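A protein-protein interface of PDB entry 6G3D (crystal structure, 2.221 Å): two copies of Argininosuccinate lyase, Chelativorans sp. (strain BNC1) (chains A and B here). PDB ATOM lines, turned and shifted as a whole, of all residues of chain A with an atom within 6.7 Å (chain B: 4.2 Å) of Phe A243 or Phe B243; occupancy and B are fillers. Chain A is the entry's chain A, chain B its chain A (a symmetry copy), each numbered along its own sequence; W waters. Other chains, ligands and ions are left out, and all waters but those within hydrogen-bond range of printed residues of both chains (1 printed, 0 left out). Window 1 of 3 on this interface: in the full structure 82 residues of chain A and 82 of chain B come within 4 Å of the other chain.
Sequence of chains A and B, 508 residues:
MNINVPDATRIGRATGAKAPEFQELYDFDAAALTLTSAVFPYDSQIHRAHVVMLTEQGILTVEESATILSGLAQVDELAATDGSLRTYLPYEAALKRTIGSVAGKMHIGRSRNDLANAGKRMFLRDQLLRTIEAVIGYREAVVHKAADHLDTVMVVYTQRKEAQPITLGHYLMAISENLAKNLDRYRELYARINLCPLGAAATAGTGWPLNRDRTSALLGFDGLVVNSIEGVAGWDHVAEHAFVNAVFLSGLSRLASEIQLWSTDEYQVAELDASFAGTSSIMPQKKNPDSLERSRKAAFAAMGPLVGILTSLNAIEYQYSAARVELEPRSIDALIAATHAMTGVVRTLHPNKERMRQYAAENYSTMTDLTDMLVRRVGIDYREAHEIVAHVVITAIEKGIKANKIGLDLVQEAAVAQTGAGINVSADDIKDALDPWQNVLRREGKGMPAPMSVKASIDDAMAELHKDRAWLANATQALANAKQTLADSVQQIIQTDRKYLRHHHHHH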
ATOM      1  N   ARG A 185      17.526   3.778   4.668  1.00  0.00           N
ATOM      2  CA  ARG A 185      18.942   4.130   4.655  1.00  0.00           C
ATOM      3  C   ARG A 185      19.798   2.983   5.178  1.00  0.00           C
ATOM      4  O   ARG A 185      20.825   2.639   4.584  1.00  0.00           O
ATOM      5  CB  ARG A 185      19.177   5.392   5.485  1.00  0.00           C
ATOM      6  CG  ARG A 185      18.536   6.640   4.923  1.00  0.00           C
ATOM      7  CD  ARG A 185      19.035   7.866   5.653  1.00  0.00           C
ATOM      8  NE  ARG A 185      18.539   9.091   5.042  1.00  0.00           N
ATOM      9  CZ  ARG A 185      17.413   9.698   5.401  1.00  0.00           C
ATOM     10  NH1 ARG A 185      16.660   9.192   6.372  1.00  0.00           N
ATOM     11  NH2 ARG A 185      17.038  10.810   4.789  1.00  0.00           N
ATOM     12  N   TYR A 186      19.384   2.371   6.289  1.00  0.00           N
ATOM     13  CA  TYR A 186      20.167   1.283   6.862  1.00  0.00           C
ATOM     14  C   TYR A 186      20.182   0.062   5.949  1.00  0.00           C
ATOM     15  O   TYR A 186      21.217  -0.602   5.808  1.00  0.00           O
ATOM     16  CB  TYR A 186      19.617   0.920   8.240  1.00  0.00           C
ATOM     17  CG  TYR A 186      20.131   1.793   9.359  1.00  0.00           C
ATOM     18  CD1 TYR A 186      21.494   1.932   9.584  1.00  0.00           C
ATOM     19  CD2 TYR A 186      19.258   2.483  10.186  1.00  0.00           C
ATOM     20  CE1 TYR A 186      21.973   2.726  10.608  1.00  0.00           C
ATOM     21  CE2 TYR A 186      19.726   3.285  11.210  1.00  0.00           C
ATOM     22  CZ  TYR A 186      21.085   3.403  11.416  1.00  0.00           C
ATOM     23  OH  TYR A 186      21.558   4.199  12.433  1.00  0.00           O
ATOM     24  N   ASP A 236      34.051   3.948   2.057  1.00  0.00           N
ATOM     25  CA  ASP A 236      32.862   4.795   2.055  1.00  0.00           C
ATOM     26  C   ASP A 236      31.732   4.187   2.873  1.00  0.00           C
ATOM     27  O   ASP A 236      30.936   4.922   3.471  1.00  0.00           O
ATOM     28  CB  ASP A 236      32.400   5.039   0.619  1.00  0.00           C
ATOM     29  CG  ASP A 236      33.393   5.861  -0.179  1.00  0.00           C
ATOM     30  OD1 ASP A 236      34.475   6.173   0.359  1.00  0.00           O
ATOM     31  OD2 ASP A 236      33.098   6.191  -1.347  1.00  0.00           O
ATOM     32  N   VAL A 238      32.024   2.715   5.624  1.00  0.00           N
ATOM     33  CA  VAL A 238      32.262   3.099   7.010  1.00  0.00           C
ATOM     34  C   VAL A 238      31.745   4.509   7.258  1.00  0.00           C
ATOM     35  O   VAL A 238      31.061   4.771   8.255  1.00  0.00           O
ATOM     36  CB  VAL A 238      33.757   2.981   7.347  1.00  0.00           C
ATOM     37  CG1 VAL A 238      33.995   3.299   8.817  1.00  0.00           C
ATOM     38  CG2 VAL A 238      34.269   1.593   6.998  1.00  0.00           C
ATOM     39  N   ALA A 239      32.062   5.437   6.350  1.00  0.00           N
ATOM     40  CA  ALA A 239      31.528   6.789   6.457  1.00  0.00           C
ATOM     41  C   ALA A 239      30.008   6.790   6.369  1.00  0.00           C
ATOM     42  O   ALA A 239      29.337   7.487   7.139  1.00  0.00           O
ATOM     43  CB  ALA A 239      32.129   7.674   5.368  1.00  0.00           C
ATOM     44  N   GLU A 240      29.445   6.005   5.443  1.00  0.00           N
ATOM     45  CA  GLU A 240      27.994   5.955   5.305  1.00  0.00           C
ATOM     46  C   GLU A 240      27.340   5.403   6.563  1.00  0.00           C
ATOM     47  O   GLU A 240      26.308   5.919   7.010  1.00  0.00           O
ATOM     48  CB  GLU A 240      27.596   5.124   4.087  1.00  0.00           C
ATOM     49  CG  GLU A 240      26.093   5.082   3.870  1.00  0.00           C
ATOM     50  CD  GLU A 240      25.698   4.384   2.592  1.00  0.00           C
ATOM     51  OE1 GLU A 240      26.601   3.914   1.870  1.00  0.00           O
ATOM     52  OE2 GLU A 240      24.483   4.303   2.313  1.00  0.00           O
ATOM     53  N   HIS A 241      27.922   4.352   7.145  1.00  0.00           N
ATOM     54  CA  HIS A 241      27.390   3.810   8.392  1.00  0.00           C
ATOM     55  C   HIS A 241      27.388   4.874   9.479  1.00  0.00           C
ATOM     56  O   HIS A 241      26.407   5.030  10.215  1.00  0.00           O
ATOM     57  CB  HIS A 241      28.204   2.588   8.824  1.00  0.00           C
ATOM     58  CG  HIS A 241      27.553   1.766   9.898  1.00  0.00           C
ATOM     59  ND1 HIS A 241      27.883   0.447  10.128  1.00  0.00           N
ATOM     60  CD2 HIS A 241      26.594   2.077  10.803  1.00  0.00           C
ATOM     61  CE1 HIS A 241      27.154  -0.018  11.128  1.00  0.00           C
ATOM     62  NE2 HIS A 241      26.365   0.951  11.556  1.00  0.00           N
ATOM     63  N   ALA A 242      28.481   5.634   9.577  1.00  0.00           N
ATOM     64  CA  ALA A 242      28.549   6.706  10.561  1.00  0.00           C
ATOM     65  C   ALA A 242      27.505   7.781  10.283  1.00  0.00           C
ATOM     66  O   ALA A 242      26.936   8.359  11.216  1.00  0.00           O
ATOM     67  CB  ALA A 242      29.955   7.307  10.579  1.00  0.00           C
ATOM     68  N   PHE A 243      27.229   8.060   9.006  1.00  0.00           N
ATOM     69  CA  PHE A 243      26.281   9.125   8.698  1.00  0.00           C
ATOM     70  C   PHE A 243      24.859   8.729   9.072  1.00  0.00           C
ATOM     71  O   PHE A 243      24.133   9.511   9.695  1.00  0.00           O
ATOM     72  CB  PHE A 243      26.325   9.515   7.226  1.00  0.00           C
ATOM     73  CG  PHE A 243      25.105  10.276   6.805  1.00  0.00           C
ATOM     74  CD1 PHE A 243      24.924  11.585   7.218  1.00  0.00           C
ATOM     75  CD2 PHE A 243      24.110   9.669   6.057  1.00  0.00           C
ATOM     76  CE1 PHE A 243      23.790  12.289   6.867  1.00  0.00           C
ATOM     77  CE2 PHE A 243      22.971  10.366   5.705  1.00  0.00           C
ATOM     78  CZ  PHE A 243      22.811  11.679   6.113  1.00  0.00           C
ATOM     79  N   VAL A 244      24.426   7.534   8.656  1.00  0.00           N
ATOM     80  CA  VAL A 244      23.057   7.114   8.941  1.00  0.00           C
ATOM     81  C   VAL A 244      22.829   7.058  10.444  1.00  0.00           C
ATOM     82  O   VAL A 244      21.761   7.437  10.940  1.00  0.00           O
ATOM     83  CB  VAL A 244      22.753   5.763   8.269  1.00  0.00           C
ATOM     84  CG1 VAL A 244      21.305   5.367   8.520  1.00  0.00           C
ATOM     85  CG2 VAL A 244      23.046   5.837   6.777  1.00  0.00           C
ATOM     86  N   ASN A 245      23.835   6.594  11.190  1.00  0.00           N
ATOM     87  CA  ASN A 245      23.796   6.685  12.643  1.00  0.00           C
ATOM     88  C   ASN A 245      23.541   8.119  13.093  1.00  0.00           C
ATOM     89  O   ASN A 245      22.714   8.371  13.976  1.00  0.00           O
ATOM     90  CB  ASN A 245      25.112   6.169  13.229  1.00  0.00           C
ATOM     91  CG  ASN A 245      25.191   4.655  13.243  1.00  0.00           C
ATOM     92  OD1 ASN A 245      24.335   3.972  12.681  1.00  0.00           O
ATOM     93  ND2 ASN A 245      26.216   4.123  13.898  1.00  0.00           N
ATOM     94  N   ALA A 246      24.237   9.076  12.477  1.00  0.00           N
ATOM     95  CA  ALA A 246      24.142  10.461  12.923  1.00  0.00           C
ATOM     96  C   ALA A 246      22.790  11.071  12.572  1.00  0.00           C
ATOM     97  O   ALA A 246      22.196  11.782  13.391  1.00  0.00           O
ATOM     98  CB  ALA A 246      25.276  11.285  12.317  1.00  0.00           C
ATOM     99  N   VAL A 247      22.282  10.808  11.363  1.00  0.00           N
ATOM    100  CA  VAL A 247      21.031  11.438  10.950  1.00  0.00           C
ATOM    101  C   VAL A 247      19.841  10.771  11.629  1.00  0.00           C
ATOM    102  O   VAL A 247      18.863  11.441  11.984  1.00  0.00           O
ATOM    103  CB  VAL A 247      20.899  11.436   9.414  1.00  0.00           C
ATOM    104  CG1 VAL A 247      20.553  10.049   8.883  1.00  0.00           C
ATOM    105  CG2 VAL A 247      19.848  12.458   8.976  1.00  0.00           C
ATOM    106  N   PHE A 248      19.902   9.450  11.832  1.00  0.00           N
ATOM    107  CA  PHE A 248      18.865   8.780  12.610  1.00  0.00           C
ATOM    108  C   PHE A 248      18.819   9.320  14.033  1.00  0.00           C
ATOM    109  O   PHE A 248      17.744   9.636  14.556  1.00  0.00           O
ATOM    110  CB  PHE A 248      19.097   7.270  12.630  1.00  0.00           C
ATOM    111  CG  PHE A 248      18.450   6.578  13.801  1.00  0.00           C
ATOM    112  CD1 PHE A 248      17.071   6.471  13.883  1.00  0.00           C
ATOM    113  CD2 PHE A 248      19.220   6.062  14.832  1.00  0.00           C
ATOM    114  CE1 PHE A 248      16.471   5.847  14.964  1.00  0.00           C
ATOM    115  CE2 PHE A 248      18.627   5.440  15.917  1.00  0.00           C
ATOM    116  CZ  PHE A 248      17.250   5.333  15.983  1.00  0.00           C
ATOM    117  N   LEU A 249      19.984   9.433  14.677  1.00  0.00           N
ATOM    118  CA  LEU A 249      20.018   9.913  16.054  1.00  0.00           C
ATOM    119  C   LEU A 249      19.582  11.369  16.159  1.00  0.00           C
ATOM    120  O   LEU A 249      19.045  11.778  17.195  1.00  0.00           O
ATOM    121  CB  LEU A 249      21.418   9.734  16.640  1.00  0.00           C
ATOM    122  CG  LEU A 249      21.767   8.316  17.083  1.00  0.00           C
ATOM    123  CD1 LEU A 249      23.258   8.189  17.317  1.00  0.00           C
ATOM    124  CD2 LEU A 249      20.995   7.966  18.341  1.00  0.00           C
ATOM    125  N   ALA A 302      27.561  11.274  18.085  1.00  0.00           N
ATOM    126  CA  ALA A 302      27.634  10.559  16.815  1.00  0.00           C
ATOM    127  C   ALA A 302      28.177  11.425  15.688  1.00  0.00           C
ATOM    128  O   ALA A 302      28.609  10.886  14.663  1.00  0.00           O
ATOM    129  CB  ALA A 302      26.255  10.019  16.437  1.00  0.00           C
ATOM    130  N   LEU A 306      31.578  10.440  12.312  1.00  0.00           N
ATOM    131  CA  LEU A 306      31.289  10.871  10.947  1.00  0.00           C
ATOM    132  C   LEU A 306      32.341  11.846  10.433  1.00  0.00           C
ATOM    133  O   LEU A 306      32.843  11.706   9.311  1.00  0.00           O
ATOM    134  CB  LEU A 306      29.899  11.506  10.893  1.00  0.00           C
ATOM    135  CG  LEU A 306      29.493  12.118   9.553  1.00  0.00           C
ATOM    136  CD1 LEU A 306      29.482  11.069   8.455  1.00  0.00           C
ATOM    137  CD2 LEU A 306      28.140  12.791   9.669  1.00  0.00           C
ATOM    138  N   LEU A 310      35.377  10.892   7.592  1.00  0.00           N
ATOM    139  CA  LEU A 310      35.438  11.640   6.340  1.00  0.00           C
ATOM    140  C   LEU A 310      36.715  12.465   6.248  1.00  0.00           C
ATOM    141  O   LEU A 310      37.297  12.598   5.166  1.00  0.00           O
ATOM    142  CB  LEU A 310      34.213  12.541   6.202  1.00  0.00           C
ATOM    143  CG  LEU A 310      32.914  11.857   5.778  1.00  0.00           C
ATOM    144  CD1 LEU A 310      31.736  12.777   6.022  1.00  0.00           C
ATOM    145  CD2 LEU A 310      32.993  11.453   4.314  1.00  0.00           C
ATOM    146  N   ALA B 239      20.282  16.709   4.912  1.00  0.00           N
ATOM    147  CA  ALA B 239      21.502  16.161   5.493  1.00  0.00           C
ATOM    148  C   ALA B 239      22.072  15.046   4.627  1.00  0.00           C
ATOM    149  O   ALA B 239      23.286  14.985   4.402  1.00  0.00           O
ATOM    150  CB  ALA B 239      21.224  15.655   6.906  1.00  0.00           C
ATOM    151  N   GLU B 240      21.207  14.157   4.122  1.00  0.00           N
ATOM    152  CA  GLU B 240      21.685  13.064   3.283  1.00  0.00           C
ATOM    153  C   GLU B 240      22.315  13.589   2.001  1.00  0.00           C
ATOM    154  O   GLU B 240      23.360  13.088   1.567  1.00  0.00           O
ATOM    155  CB  GLU B 240      20.548  12.095   2.962  1.00  0.00           C
ATOM    156  CG  GLU B 240      21.004  10.909   2.128  1.00  0.00           C
ATOM    157  CD  GLU B 240      19.923   9.876   1.925  1.00  0.00           C
ATOM    158  OE1 GLU B 240      18.801  10.088   2.427  1.00  0.00           O
ATOM    159  OE2 GLU B 240      20.199   8.855   1.262  1.00  0.00           O
ATOM    160  N   HIS B 241      21.693  14.594   1.379  1.00  0.00           N
ATOM    161  CA  HIS B 241      22.275  15.192   0.182  1.00  0.00           C
ATOM    162  C   HIS B 241      23.658  15.750   0.481  1.00  0.00           C
ATOM    163  O   HIS B 241      24.604  15.552  -0.291  1.00  0.00           O
ATOM    164  CB  HIS B 241      21.350  16.286  -0.360  1.00  0.00           C
ATOM    165  CG  HIS B 241      21.684  16.736  -1.754  1.00  0.00           C
ATOM    166  ND1 HIS B 241      20.770  17.370  -2.569  1.00  0.00           N
ATOM    167  CD2 HIS B 241      22.828  16.642  -2.472  1.00  0.00           C
ATOM    168  CE1 HIS B 241      21.339  17.647  -3.729  1.00  0.00           C
ATOM    169  NE2 HIS B 241      22.587  17.216  -3.697  1.00  0.00           N
ATOM    170  N   ALA B 242      23.797  16.434   1.619  1.00  0.00           N
ATOM    171  CA  ALA B 242      25.096  16.966   2.007  1.00  0.00           C
ATOM    172  C   ALA B 242      26.103  15.848   2.248  1.00  0.00           C
ATOM    173  O   ALA B 242      27.290  15.995   1.934  1.00  0.00           O
ATOM    174  CB  ALA B 242      24.949  17.842   3.251  1.00  0.00           C
ATOM    175  N   PHE B 243      25.652  14.716   2.795  1.00  0.00           N
ATOM    176  CA  PHE B 243      26.596  13.646   3.098  1.00  0.00           C
ATOM    177  C   PHE B 243      27.124  12.993   1.828  1.00  0.00           C
ATOM    178  O   PHE B 243      28.333  12.778   1.690  1.00  0.00           O
ATOM    179  CB  PHE B 243      25.975  12.580   3.992  1.00  0.00           C
ATOM    180  CG  PHE B 243      26.752  11.298   3.968  1.00  0.00           C
ATOM    181  CD1 PHE B 243      27.979  11.216   4.605  1.00  0.00           C
ATOM    182  CD2 PHE B 243      26.293  10.201   3.258  1.00  0.00           C
ATOM    183  CE1 PHE B 243      28.722  10.054   4.564  1.00  0.00           C
ATOM    184  CE2 PHE B 243      27.034   9.036   3.210  1.00  0.00           C
ATOM    185  CZ  PHE B 243      28.252   8.964   3.864  1.00  0.00           C
ATOM    186  N   VAL B 244      26.226  12.627   0.908  1.00  0.00           N
ATOM    187  CA  VAL B 244      26.663  11.954  -0.312  1.00  0.00           C
ATOM    188  C   VAL B 244      27.608  12.852  -1.094  1.00  0.00           C
ATOM    189  O   VAL B 244      28.603  12.385  -1.665  1.00  0.00           O
ATOM    190  CB  VAL B 244      25.452  11.527  -1.160  1.00  0.00           C
ATOM    191  CG1 VAL B 244      25.917  10.771  -2.397  1.00  0.00           C
ATOM    192  CG2 VAL B 244      24.498  10.679  -0.331  1.00  0.00           C
ATOM    193  N   ASN B 245      27.318  14.155  -1.123  1.00  0.00           N
ATOM    194  CA  ASN B 245      28.259  15.123  -1.671  1.00  0.00           C
ATOM    195  C   ASN B 245      29.625  14.991  -1.006  1.00  0.00           C
ATOM    196  O   ASN B 245      30.662  14.985  -1.679  1.00  0.00           O
ATOM    197  CB  ASN B 245      27.711  16.539  -1.486  1.00  0.00           C
ATOM    198  CG  ASN B 245      26.637  16.886  -2.498  1.00  0.00           C
ATOM    199  OD1 ASN B 245      26.180  16.028  -3.254  1.00  0.00           O
ATOM    200  ND2 ASN B 245      26.238  18.151  -2.526  1.00  0.00           N
ATOM    201  N   ALA B 246      29.639  14.867   0.322  1.00  0.00           N
ATOM    202  CA  ALA B 246      30.903  14.853   1.049  1.00  0.00           C
ATOM    203  C   ALA B 246      31.670  13.557   0.813  1.00  0.00           C
ATOM    204  O   ALA B 246      32.893  13.583   0.624  1.00  0.00           O
ATOM    205  CB  ALA B 246      30.652  15.065   2.540  1.00  0.00           C
ATOM    206  N   VAL B 247      30.978  12.413   0.818  1.00  0.00           N
ATOM    207  CA  VAL B 247      31.681  11.140   0.682  1.00  0.00           C
ATOM    208  C   VAL B 247      32.109  10.912  -0.763  1.00  0.00           C
ATOM    209  O   VAL B 247      33.183  10.355  -1.021  1.00  0.00           O
ATOM    210  CB  VAL B 247      30.823   9.980   1.224  1.00  0.00           C
ATOM    211  CG1 VAL B 247      29.687   9.630   0.268  1.00  0.00           C
ATOM    212  CG2 VAL B 247      31.702   8.757   1.489  1.00  0.00           C
ATOM    213  N   LEU B 306      27.486  19.589   5.692  1.00  0.00           N
ATOM    214  CA  LEU B 306      27.094  18.358   6.373  1.00  0.00           C
ATOM    215  C   LEU B 306      27.036  18.549   7.884  1.00  0.00           C
ATOM    216  O   LEU B 306      26.067  18.143   8.539  1.00  0.00           O
ATOM    217  CB  LEU B 306      28.070  17.238   6.013  1.00  0.00           C
ATOM    218  CG  LEU B 306      27.866  15.911   6.740  1.00  0.00           C
ATOM    219  CD1 LEU B 306      26.491  15.335   6.448  1.00  0.00           C
ATOM    220  CD2 LEU B 306      28.955  14.928   6.359  1.00  0.00           C
HETATM  221  O   HOH W   1      33.686   8.383  -2.597  1.00  0.00           O
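Ala A239 touches Phe B243, and with the chains exchanged Phe A243 touches Ala B239. Glu A240 touches Phe B243, and with the chains exchanged Phe A243 touches Glu B240. Phe B243 touches its own counterpart, Phe A243. Of the 9 pairs that touch across the chains among the printed residues, 5 have their exchanged pair printed and touching as well.
Water W1 lies within hydrogen-bond range of O of Val B247 and OD2 of Asp A236.
Of the 18 printed residues of chain A, 6 touch a printed residue of chain B. Along chain A the printed residues that touch a printed residue of chain B span positions 185 to 310. Hydrophobic or aromatic side chains of chain B that line the printed part of chain A: Phe B243, Val B247 and Leu B306.
The guanidinium group (NE) of Arg A185 lies within salt-bridge range of the side-chain carboxylate (OE1) of Glu B240 (2.8 Å).
Of the printed residues of chain B, Arg A185 touches Glu B240 (2.8 Å). Printed residues of chain B within 4 Å of Glu A240: Phe B243 (3.3 Å). Printed residues of chain A within 4 Å of Ala B239: Phe A243 (3.7 Å). Ala B242 touches none of the printed residues of chain A. Phe B243 touches just these residues of chain A: Ala A239, Glu A240 and Phe A243. Of the printed residues of chain A, Leu B306 touches Leu A310 (3.5 Å). The nearest residue of chain B that does not touch Phe A243 is Leu B306 (4.1 Å). The nearest residue of chain A that does not touch Phe B243 is Leu A306 (4.1 Å). The nearest printed residue of chain A that does not touch Ala B239 is Val A247 (4.05 Å).
Val B247 touches Asp A236. Ala A239 touches Phe B243. CA of Glu A240 touches CZ of Phe B243, 3.3 Å away. CE1 of Phe A243 touches O of Ala B239 (3.7 Å). Phe A243 touches Glu B240. CG of Phe B243 touches CG of Phe A243, 3.4 Å away. Val B247 touches Leu A310. Leu A310 touches Leu B306 (CD1 to CD2, 3.5 Å).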
